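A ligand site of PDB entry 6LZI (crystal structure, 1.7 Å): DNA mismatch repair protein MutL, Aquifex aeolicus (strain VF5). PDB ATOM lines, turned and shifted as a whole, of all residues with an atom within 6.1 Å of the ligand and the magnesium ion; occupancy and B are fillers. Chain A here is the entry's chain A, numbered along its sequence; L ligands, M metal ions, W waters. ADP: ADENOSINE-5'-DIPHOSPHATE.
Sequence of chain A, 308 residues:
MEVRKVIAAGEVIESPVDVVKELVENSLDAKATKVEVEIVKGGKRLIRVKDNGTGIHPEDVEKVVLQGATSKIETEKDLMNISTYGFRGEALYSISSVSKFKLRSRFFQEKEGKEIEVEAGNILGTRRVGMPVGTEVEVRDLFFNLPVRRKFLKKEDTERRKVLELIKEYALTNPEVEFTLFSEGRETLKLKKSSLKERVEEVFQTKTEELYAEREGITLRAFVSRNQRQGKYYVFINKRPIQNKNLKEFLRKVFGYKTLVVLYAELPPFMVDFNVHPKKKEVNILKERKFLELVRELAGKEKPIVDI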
ATOM      1  N   GLU A  22       4.398  25.821   0.112  1.00  0.00           N
ATOM      2  CA  GLU A  22       5.058  25.264  -1.072  1.00  0.00           C
ATOM      3  C   GLU A  22       5.968  26.273  -1.652  1.00  0.00           C
ATOM      4  O   GLU A  22       7.093  25.915  -2.037  1.00  0.00           O
ATOM      5  CB  GLU A  22       4.079  24.792  -2.113  1.00  0.00           C
ATOM      6  CG  GLU A  22       3.149  23.720  -1.577  1.00  0.00           C
ATOM      7  CD  GLU A  22       3.864  22.402  -1.286  1.00  0.00           C
ATOM      8  OE1 GLU A  22       3.367  21.585  -0.468  1.00  0.00           O
ATOM      9  OE2 GLU A  22       4.950  22.189  -1.833  1.00  0.00           O
ATOM     10  N   LEU A  23       5.555  27.562  -1.688  1.00  0.00           N
ATOM     11  CA  LEU A  23       6.478  28.531  -2.296  1.00  0.00           C
ATOM     12  C   LEU A  23       7.733  28.730  -1.443  1.00  0.00           C
ATOM     13  O   LEU A  23       8.843  28.774  -1.971  1.00  0.00           O
ATOM     14  CB  LEU A  23       5.774  29.876  -2.570  1.00  0.00           C
ATOM     15  CG  LEU A  23       4.641  29.594  -3.566  1.00  0.00           C
ATOM     16  CD1 LEU A  23       3.868  30.981  -3.747  1.00  0.00           C
ATOM     17  CD2 LEU A  23       4.970  28.994  -4.895  1.00  0.00           C
ATOM     18  N   GLU A  25       9.055  26.762   0.694  1.00  0.00           N
ATOM     19  CA  GLU A  25       9.888  25.559   0.578  1.00  0.00           C
ATOM     20  C   GLU A  25      10.743  25.618  -0.680  1.00  0.00           C
ATOM     21  O   GLU A  25      11.945  25.300  -0.627  1.00  0.00           O
ATOM     22  CB  GLU A  25       9.017  24.284   0.613  1.00  0.00           C
ATOM     23  CG  GLU A  25       9.817  22.993   0.377  1.00  0.00           C
ATOM     24  CD  GLU A  25       8.941  21.755   0.542  1.00  0.00           C
ATOM     25  OE1 GLU A  25       8.782  20.904  -0.408  1.00  0.00           O
ATOM     26  OE2 GLU A  25       8.447  21.588   1.663  1.00  0.00           O
ATOM     27  N   ASN A  26      10.170  26.105  -1.809  1.00  0.00           N
ATOM     28  CA  ASN A  26      10.889  26.170  -3.073  1.00  0.00           C
ATOM     29  C   ASN A  26      11.993  27.209  -2.976  1.00  0.00           C
ATOM     30  O   ASN A  26      13.119  26.982  -3.472  1.00  0.00           O
ATOM     31  CB  ASN A  26       9.913  26.510  -4.206  1.00  0.00           C
ATOM     32  CG  ASN A  26       9.111  25.297  -4.617  1.00  0.00           C
ATOM     33  OD1 ASN A  26       9.497  24.183  -4.271  1.00  0.00           O
ATOM     34  ND2 ASN A  26       8.057  25.473  -5.359  1.00  0.00           N
ATOM     35  N   SER A  27      11.722  28.297  -2.286  1.00  0.00           N
ATOM     36  CA  SER A  27      12.785  29.304  -2.128  1.00  0.00           C
ATOM     37  C   SER A  27      13.960  28.752  -1.373  1.00  0.00           C
ATOM     38  O   SER A  27      15.109  29.046  -1.706  1.00  0.00           O
ATOM     39  CB  SER A  27      12.282  30.496  -1.368  1.00  0.00           C
ATOM     40  OG  SER A  27      11.209  31.061  -2.164  1.00  0.00           O
ATOM     41  N   ASP A  29      14.739  25.571  -0.925  1.00  0.00           N
ATOM     42  CA  ASP A  29      15.359  24.580  -1.800  1.00  0.00           C
ATOM     43  C   ASP A  29      16.334  25.227  -2.771  1.00  0.00           C
ATOM     44  O   ASP A  29      17.372  24.642  -3.079  1.00  0.00           O
ATOM     45  CB  ASP A  29      14.319  23.801  -2.606  1.00  0.00           C
ATOM     46  CG  ASP A  29      13.474  22.813  -1.778  1.00  0.00           C
ATOM     47  OD1 ASP A  29      13.783  22.499  -0.600  1.00  0.00           O
ATOM     48  OD2 ASP A  29      12.444  22.400  -2.356  1.00  0.00           O
ATOM     49  N   ALA A  30      16.029  26.440  -3.233  1.00  0.00           N
ATOM     50  CA  ALA A  30      16.888  27.173  -4.162  1.00  0.00           C
ATOM     51  C   ALA A  30      17.911  28.060  -3.450  1.00  0.00           C
ATOM     52  O   ALA A  30      18.510  28.933  -4.094  1.00  0.00           O
ATOM     53  CB  ALA A  30      16.053  28.015  -5.099  1.00  0.00           C
ATOM     54  N   ASP A  51      12.199  35.634  -3.589  1.00  0.00           N
ATOM     55  CA  ASP A  51      13.458  35.146  -3.033  1.00  0.00           C
ATOM     56  C   ASP A  51      14.637  35.574  -3.905  1.00  0.00           C
ATOM     57  O   ASP A  51      14.487  35.967  -5.085  1.00  0.00           O
ATOM     58  CB  ASP A  51      13.419  33.584  -2.864  1.00  0.00           C
ATOM     59  CG  ASP A  51      13.511  32.820  -4.166  1.00  0.00           C
ATOM     60  OD1 ASP A  51      14.459  33.057  -4.996  1.00  0.00           O
ATOM     61  OD2 ASP A  51      12.573  31.985  -4.410  1.00  0.00           O
ATOM     62  N   GLY A  53      17.274  33.446  -4.402  1.00  0.00           N
ATOM     63  CA  GLY A  53      17.957  32.200  -4.703  1.00  0.00           C
ATOM     64  C   GLY A  53      18.503  32.153  -6.112  1.00  0.00           C
ATOM     65  O   GLY A  53      18.597  33.160  -6.828  1.00  0.00           O
ATOM     66  N   THR A  54      18.807  30.950  -6.531  1.00  0.00           N
ATOM     67  CA  THR A  54      19.550  30.787  -7.772  1.00  0.00           C
ATOM     68  C   THR A  54      18.703  31.041  -9.005  1.00  0.00           C
ATOM     69  O   THR A  54      19.251  31.094 -10.105  1.00  0.00           O
ATOM     70  CB  THR A  54      20.116  29.357  -7.848  1.00  0.00           C
ATOM     71  OG1 THR A  54      19.041  28.454  -8.164  1.00  0.00           O
ATOM     72  CG2 THR A  54      20.629  28.964  -6.535  1.00  0.00           C
ATOM     73  N   GLY A  55      17.373  31.108  -8.850  1.00  0.00           N
ATOM     74  CA  GLY A  55      16.503  31.262 -10.003  1.00  0.00           C
ATOM     75  C   GLY A  55      16.423  30.004 -10.879  1.00  0.00           C
ATOM     76  O   GLY A  55      16.859  28.909 -10.531  1.00  0.00           O
ATOM     77  N   ILE A  56      15.734  30.206 -12.001  1.00  0.00           N
ATOM     78  CA  ILE A  56      15.350  29.136 -12.909  1.00  0.00           C
ATOM     79  C   ILE A  56      15.783  29.576 -14.297  1.00  0.00           C
ATOM     80  O   ILE A  56      15.559  30.742 -14.659  1.00  0.00           O
ATOM     81  CB  ILE A  56      13.832  28.845 -12.860  1.00  0.00           C
ATOM     82  CG1 ILE A  56      13.408  28.540 -11.410  1.00  0.00           C
ATOM     83  CG2 ILE A  56      13.456  27.663 -13.770  1.00  0.00           C
ATOM     84  CD1 ILE A  56      11.964  28.881 -11.124  1.00  0.00           C
ATOM     85  N   LYS A  63       8.457  24.701 -18.052  1.00  0.00           N
ATOM     86  CA  LYS A  63       8.325  23.327 -17.570  1.00  0.00           C
ATOM     87  C   LYS A  63       7.696  23.251 -16.179  1.00  0.00           C
ATOM     88  O   LYS A  63       6.905  22.341 -15.903  1.00  0.00           O
ATOM     89  CB  LYS A  63       9.717  22.682 -17.602  1.00  0.00           C
ATOM     90  CG  LYS A  63       9.817  21.194 -17.337  1.00  0.00           C
ATOM     91  CD  LYS A  63      10.079  20.918 -15.853  1.00  0.00           C
ATOM     92  CE  LYS A  63      11.241  21.762 -15.327  1.00  0.00           C
ATOM     93  NZ  LYS A  63      11.139  22.007 -13.865  1.00  0.00           N
ATOM     94  N   VAL A  64       8.027  24.188 -15.294  1.00  0.00           N
ATOM     95  CA  VAL A  64       7.670  24.032 -13.892  1.00  0.00           C
ATOM     96  C   VAL A  64       6.188  24.199 -13.627  1.00  0.00           C
ATOM     97  O   VAL A  64       5.738  23.882 -12.514  1.00  0.00           O
ATOM     98  CB  VAL A  64       8.471  25.020 -13.007  1.00  0.00           C
ATOM     99  CG1 VAL A  64       9.954  24.853 -13.242  1.00  0.00           C
ATOM    100  CG2 VAL A  64       8.033  26.453 -13.280  1.00  0.00           C
ATOM    101  N   GLU A  90       3.066  18.270  -9.759  1.00  0.00           N
ATOM    102  CA  GLU A  90       3.967  18.796  -8.765  1.00  0.00           C
ATOM    103  C   GLU A  90       3.329  20.026  -8.156  1.00  0.00           C
ATOM    104  O   GLU A  90       2.187  20.372  -8.468  1.00  0.00           O
ATOM    105  CB  GLU A  90       5.328  19.102  -9.358  1.00  0.00           C
ATOM    106  CG  GLU A  90       6.426  18.065  -9.145  1.00  0.00           C
ATOM    107  CD  GLU A  90       7.749  18.467  -9.836  1.00  0.00           C
ATOM    108  OE1 GLU A  90       7.769  19.561 -10.471  1.00  0.00           O
ATOM    109  OE2 GLU A  90       8.764  17.725  -9.748  1.00  0.00           O
ATOM    110  N   ALA A  91       4.077  20.715  -7.296  1.00  0.00           N
ATOM    111  CA  ALA A  91       3.424  21.677  -6.430  1.00  0.00           C
ATOM    112  C   ALA A  91       3.012  22.926  -7.221  1.00  0.00           C
ATOM    113  O   ALA A  91       1.883  23.409  -7.061  1.00  0.00           O
ATOM    114  CB  ALA A  91       4.334  22.018  -5.232  1.00  0.00           C
ATOM    115  N   LEU A  92       3.905  23.467  -8.101  1.00  0.00           N
ATOM    116  CA  LEU A  92       3.459  24.672  -8.827  1.00  0.00           C
ATOM    117  C   LEU A  92       2.329  24.397  -9.799  1.00  0.00           C
ATOM    118  O   LEU A  92       1.526  25.315 -10.116  1.00  0.00           O
ATOM    119  CB  LEU A  92       4.626  25.314  -9.569  1.00  0.00           C
ATOM    120  CG  LEU A  92       5.711  25.770  -8.629  1.00  0.00           C
ATOM    121  CD1 LEU A  92       6.962  26.215  -9.423  1.00  0.00           C
ATOM    122  CD2 LEU A  92       5.222  26.964  -7.789  1.00  0.00           C
ATOM    123  N   TYR A  93       2.296  23.195 -10.376  1.00  0.00           N
ATOM    124  CA  TYR A  93       1.191  22.849 -11.257  1.00  0.00           C
ATOM    125  C   TYR A  93      -0.110  22.912 -10.496  1.00  0.00           C
ATOM    126  O   TYR A  93      -1.125  23.436 -10.978  1.00  0.00           O
ATOM    127  CB  TYR A  93       1.373  21.446 -11.788  1.00  0.00           C
ATOM    128  CG  TYR A  93       0.176  20.942 -12.531  1.00  0.00           C
ATOM    129  CD1 TYR A  93      -0.127  21.408 -13.780  1.00  0.00           C
ATOM    130  CD2 TYR A  93      -0.647  19.979 -11.956  1.00  0.00           C
ATOM    131  CE1 TYR A  93      -1.251  20.935 -14.459  1.00  0.00           C
ATOM    132  CE2 TYR A  93      -1.762  19.485 -12.642  1.00  0.00           C
ATOM    133  CZ  TYR A  93      -2.054  19.977 -13.875  1.00  0.00           C
ATOM    134  OH  TYR A  93      -3.168  19.482 -14.531  1.00  0.00           O
ATOM    135  N   LEU A 103       4.689  33.451 -12.496  1.00  0.00           N
ATOM    136  CA  LEU A 103       6.008  33.175 -11.919  1.00  0.00           C
ATOM    137  C   LEU A 103       7.040  33.904 -12.741  1.00  0.00           C
ATOM    138  O   LEU A 103       7.070  33.745 -13.955  1.00  0.00           O
ATOM    139  CB  LEU A 103       6.329  31.701 -11.925  1.00  0.00           C
ATOM    140  CG  LEU A 103       7.739  31.189 -11.472  1.00  0.00           C
ATOM    141  CD1 LEU A 103       7.676  29.776 -10.763  1.00  0.00           C
ATOM    142  CD2 LEU A 103       8.700  31.079 -12.581  1.00  0.00           C
ATOM    143  N   SER A 105      11.307  34.635 -12.971  1.00  0.00           N
ATOM    144  CA  SER A 105      12.592  34.148 -12.439  1.00  0.00           C
ATOM    145  C   SER A 105      13.762  34.557 -13.335  1.00  0.00           C
ATOM    146  O   SER A 105      13.681  34.521 -14.570  1.00  0.00           O
ATOM    147  CB  SER A 105      12.604  32.612 -12.275  1.00  0.00           C
ATOM    148  OG  SER A 105      13.745  32.187 -11.567  1.00  0.00           O
ATOM    149  N   GLY A 134      16.874  35.704  -8.948  1.00  0.00           N
ATOM    150  CA  GLY A 134      15.998  35.015  -8.004  1.00  0.00           C
ATOM    151  C   GLY A 134      14.601  34.794  -8.622  1.00  0.00           C
ATOM    152  O   GLY A 134      14.438  34.782  -9.847  1.00  0.00           O
ATOM    153  N   THR A 135      13.606  34.569  -7.774  1.00  0.00           N
ATOM    154  CA  THR A 135      12.286  34.099  -8.232  1.00  0.00           C
ATOM    155  C   THR A 135      11.191  34.796  -7.463  1.00  0.00           C
ATOM    156  O   THR A 135      11.324  35.039  -6.274  1.00  0.00           O
ATOM    157  CB  THR A 135      12.166  32.560  -8.023  1.00  0.00           C
ATOM    158  OG1 THR A 135      13.209  31.911  -8.749  1.00  0.00           O
ATOM    159  CG2 THR A 135      10.839  32.020  -8.484  1.00  0.00           C
ATOM    160  N   VAL A 137       6.852  34.594  -7.203  1.00  0.00           N
ATOM    161  CA  VAL A 137       5.629  33.910  -7.607  1.00  0.00           C
ATOM    162  C   VAL A 137       4.465  34.704  -7.031  1.00  0.00           C
ATOM    163  O   VAL A 137       4.491  35.109  -5.849  1.00  0.00           O
ATOM    164  CB  VAL A 137       5.659  32.449  -7.069  1.00  0.00           C
ATOM    165  CG1 VAL A 137       4.396  31.682  -7.560  1.00  0.00           C
ATOM    166  CG2 VAL A 137       6.908  31.803  -7.599  1.00  0.00           C
HETATM  167  PB  ADP L   1       9.400  20.277  -6.395  1.00  0.00           P
HETATM  168  O1B ADP L   1       9.860  21.466  -5.611  1.00  0.00           O
HETATM  169  O2B ADP L   1      10.500  19.765  -7.365  1.00  0.00           O
HETATM  170  O3B ADP L   1       8.923  19.153  -5.493  1.00  0.00           O
HETATM  171  PA  ADP L   1       7.649  22.278  -7.448  1.00  0.00           P
HETATM  172  O1A ADP L   1       6.429  22.206  -8.334  1.00  0.00           O
HETATM  173  O2A ADP L   1       7.430  22.920  -6.126  1.00  0.00           O
HETATM  174  O3A ADP L   1       8.171  20.712  -7.307  1.00  0.00           O
HETATM  175  O5' ADP L   1       8.792  23.182  -8.145  1.00  0.00           O
HETATM  176  C5' ADP L   1       9.221  22.580  -9.364  1.00  0.00           C
HETATM  177  C4' ADP L   1      10.657  22.992  -9.689  1.00  0.00           C
HETATM  178  O4' ADP L   1      10.678  24.367  -9.980  1.00  0.00           O
HETATM  179  C3' ADP L   1      11.683  22.786  -8.593  1.00  0.00           C
HETATM  180  O3' ADP L   1      12.265  21.461  -8.715  1.00  0.00           O
HETATM  181  C2' ADP L   1      12.730  23.831  -8.924  1.00  0.00           C
HETATM  182  O2' ADP L   1      13.530  23.200  -9.981  1.00  0.00           O
HETATM  183  C1' ADP L   1      11.915  24.926  -9.575  1.00  0.00           C
HETATM  184  N9  ADP L   1      11.582  26.003  -8.653  1.00  0.00           N
HETATM  185  C8  ADP L   1      10.377  26.271  -8.083  1.00  0.00           C
HETATM  186  N7  ADP L   1      10.445  27.387  -7.292  1.00  0.00           N
HETATM  187  C5  ADP L   1      11.738  27.787  -7.372  1.00  0.00           C
HETATM  188  C6  ADP L   1      12.471  28.895  -6.760  1.00  0.00           C
HETATM  189  N6  ADP L   1      11.833  29.740  -5.899  1.00  0.00           N
HETATM  190  N1  ADP L   1      13.794  29.012  -7.058  1.00  0.00           N
HETATM  191  C2  ADP L   1      14.402  28.093  -7.915  1.00  0.00           C
HETATM  192  N3  ADP L   1      13.790  27.078  -8.520  1.00  0.00           N
HETATM  193  C4  ADP L   1      12.470  26.918  -8.269  1.00  0.00           C
HETATM  194 MG    MG M   1       8.525  22.399  -4.340  1.00  0.00          MG
HETATM  195  O   HOH W   1      15.086  31.354  -6.936  1.00  0.00           O
HETATM  196  O   HOH W   2       6.950  23.450  -3.198  1.00  0.00           O
HETATM  197  O   HOH W   3       9.171  30.089  -4.520  1.00  0.00           O
HETATM  198  O   HOH W   4      14.262  20.820  -6.427  1.00  0.00           O
HETATM  199  O   HOH W   5       7.290  20.592  -4.216  1.00  0.00           O
HETATM  200  O   HOH W   6      11.384  17.045  -7.364  1.00  0.00           O
HETATM  201  O   HOH W   7       9.652  21.825  -2.743  1.00  0.00           O
HETATM  202  O   HOH W   8      12.337  22.623  -5.061  1.00  0.00           O
HETATM  203  O   HOH W   9      15.750  25.626  -9.776  1.00  0.00           O
HETATM  204  O   HOH W  10       4.833  21.629 -10.811  1.00  0.00           O
HETATM  205  O   HOH W  11      13.420  19.950 -10.198  1.00  0.00           O
HETATM  206  O   HOH W  12       8.025  28.166  -6.216  1.00  0.00           O
HETATM  207  O   HOH W  13       8.763  17.740  -2.779  1.00  0.00           O
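The magnesium ion is bound by OD1 of Asn 26 (2.0 Å), water W7 (2.0 Å), O1B of the ligand (2.1 Å), O2A of the ligand (2.2 Å), water W5 (2.2 Å) and water W2 (2.2 Å).
ND2 of Asn 26 sits close to O of Glu 22 (3.5 Å). O of Thr 135 is in hydrogen-bond range of N of Asp 51 (2.9 Å). The side-chain hydroxyl (OG) of Ser 27 sits at hydrogen-bond distance from the side-chain carboxylate (OD2) of Asp 51, 2.8 Å away. The side-chain carboxylate of Asp 51 sits at hydrogen-bond distance from the backbone NH of Gly 53 (2.9 Å). The backbone NH of Thr 54 lies within hydrogen-bond range of the backbone carbonyl oxygen of Ala 30 (3.2 Å). N of Ile 56 is in hydrogen-bond range of OG of Ser 105. The side-chain hydroxyl of Thr 135 is in hydrogen-bond range of the side-chain hydroxyl of Ser 105 (2.9 Å). O of Leu 23 is in hydrogen-bond range of OG of Ser 27 (3.3 Å).
OD2 of Asp 51 lies within hydrogen-bond range of N6 of the ligand, 2.8 Å away. The backbone NH (N) of Leu 92 lies within hydrogen-bond range of an oxygen (O1A) of the ligand. The backbone NH (N) of Ala 91 sits at hydrogen-bond distance from an oxygen (O1A) of the ligand, at 3.0 Å. The side-chain hydroxyl of Thr 135 lies within hydrogen-bond range of a nitrogen (N1) of the ligand, at 3.4 Å.
Water W7 lies within hydrogen-bond range of the side-chain carboxylate (OE1) of Glu 25 (2.7 Å) and the side-chain carboxylate (OD2) of Asp 29 (2.9 Å). Water W2 lies within hydrogen-bond range of O of Glu 22 and ND2 of Asn 26. Water W1 lies within hydrogen-bond range of the side-chain carboxylate (OD1) of Asp 51, the side-chain hydroxyl (OG1) of Thr 135, a nitrogen (N1) of the ligand and the backbone NH (N) of Gly 55. Water W12 bridges a nitrogen (N7) of the ligand and the side-chain amide nitrogen of Asn 26. Water W10 lies within hydrogen-bond range of the backbone carbonyl oxygen of Val 64, an oxygen (O1A) of the ligand, the backbone NH of Tyr 93 and the backbone NH of Leu 92. Water W3 lies within hydrogen-bond range of O of Leu 23, N6 of the ligand and OG of Ser 27.
The side-chain carboxylate of Glu 90 lies close to an oxygen (O3A) of the ligand, at 3.4 Å. Merely in contact with the ligand: Ala 30 (3.2 Å), Ile 56 (3.3 Å), Val 64 (3.4 Å), Gly 55 (3.7 Å) and Ser 27 (3.9 Å). The nearest printed residue that does not touch the ligand is Asp 29 (4.3 Å).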
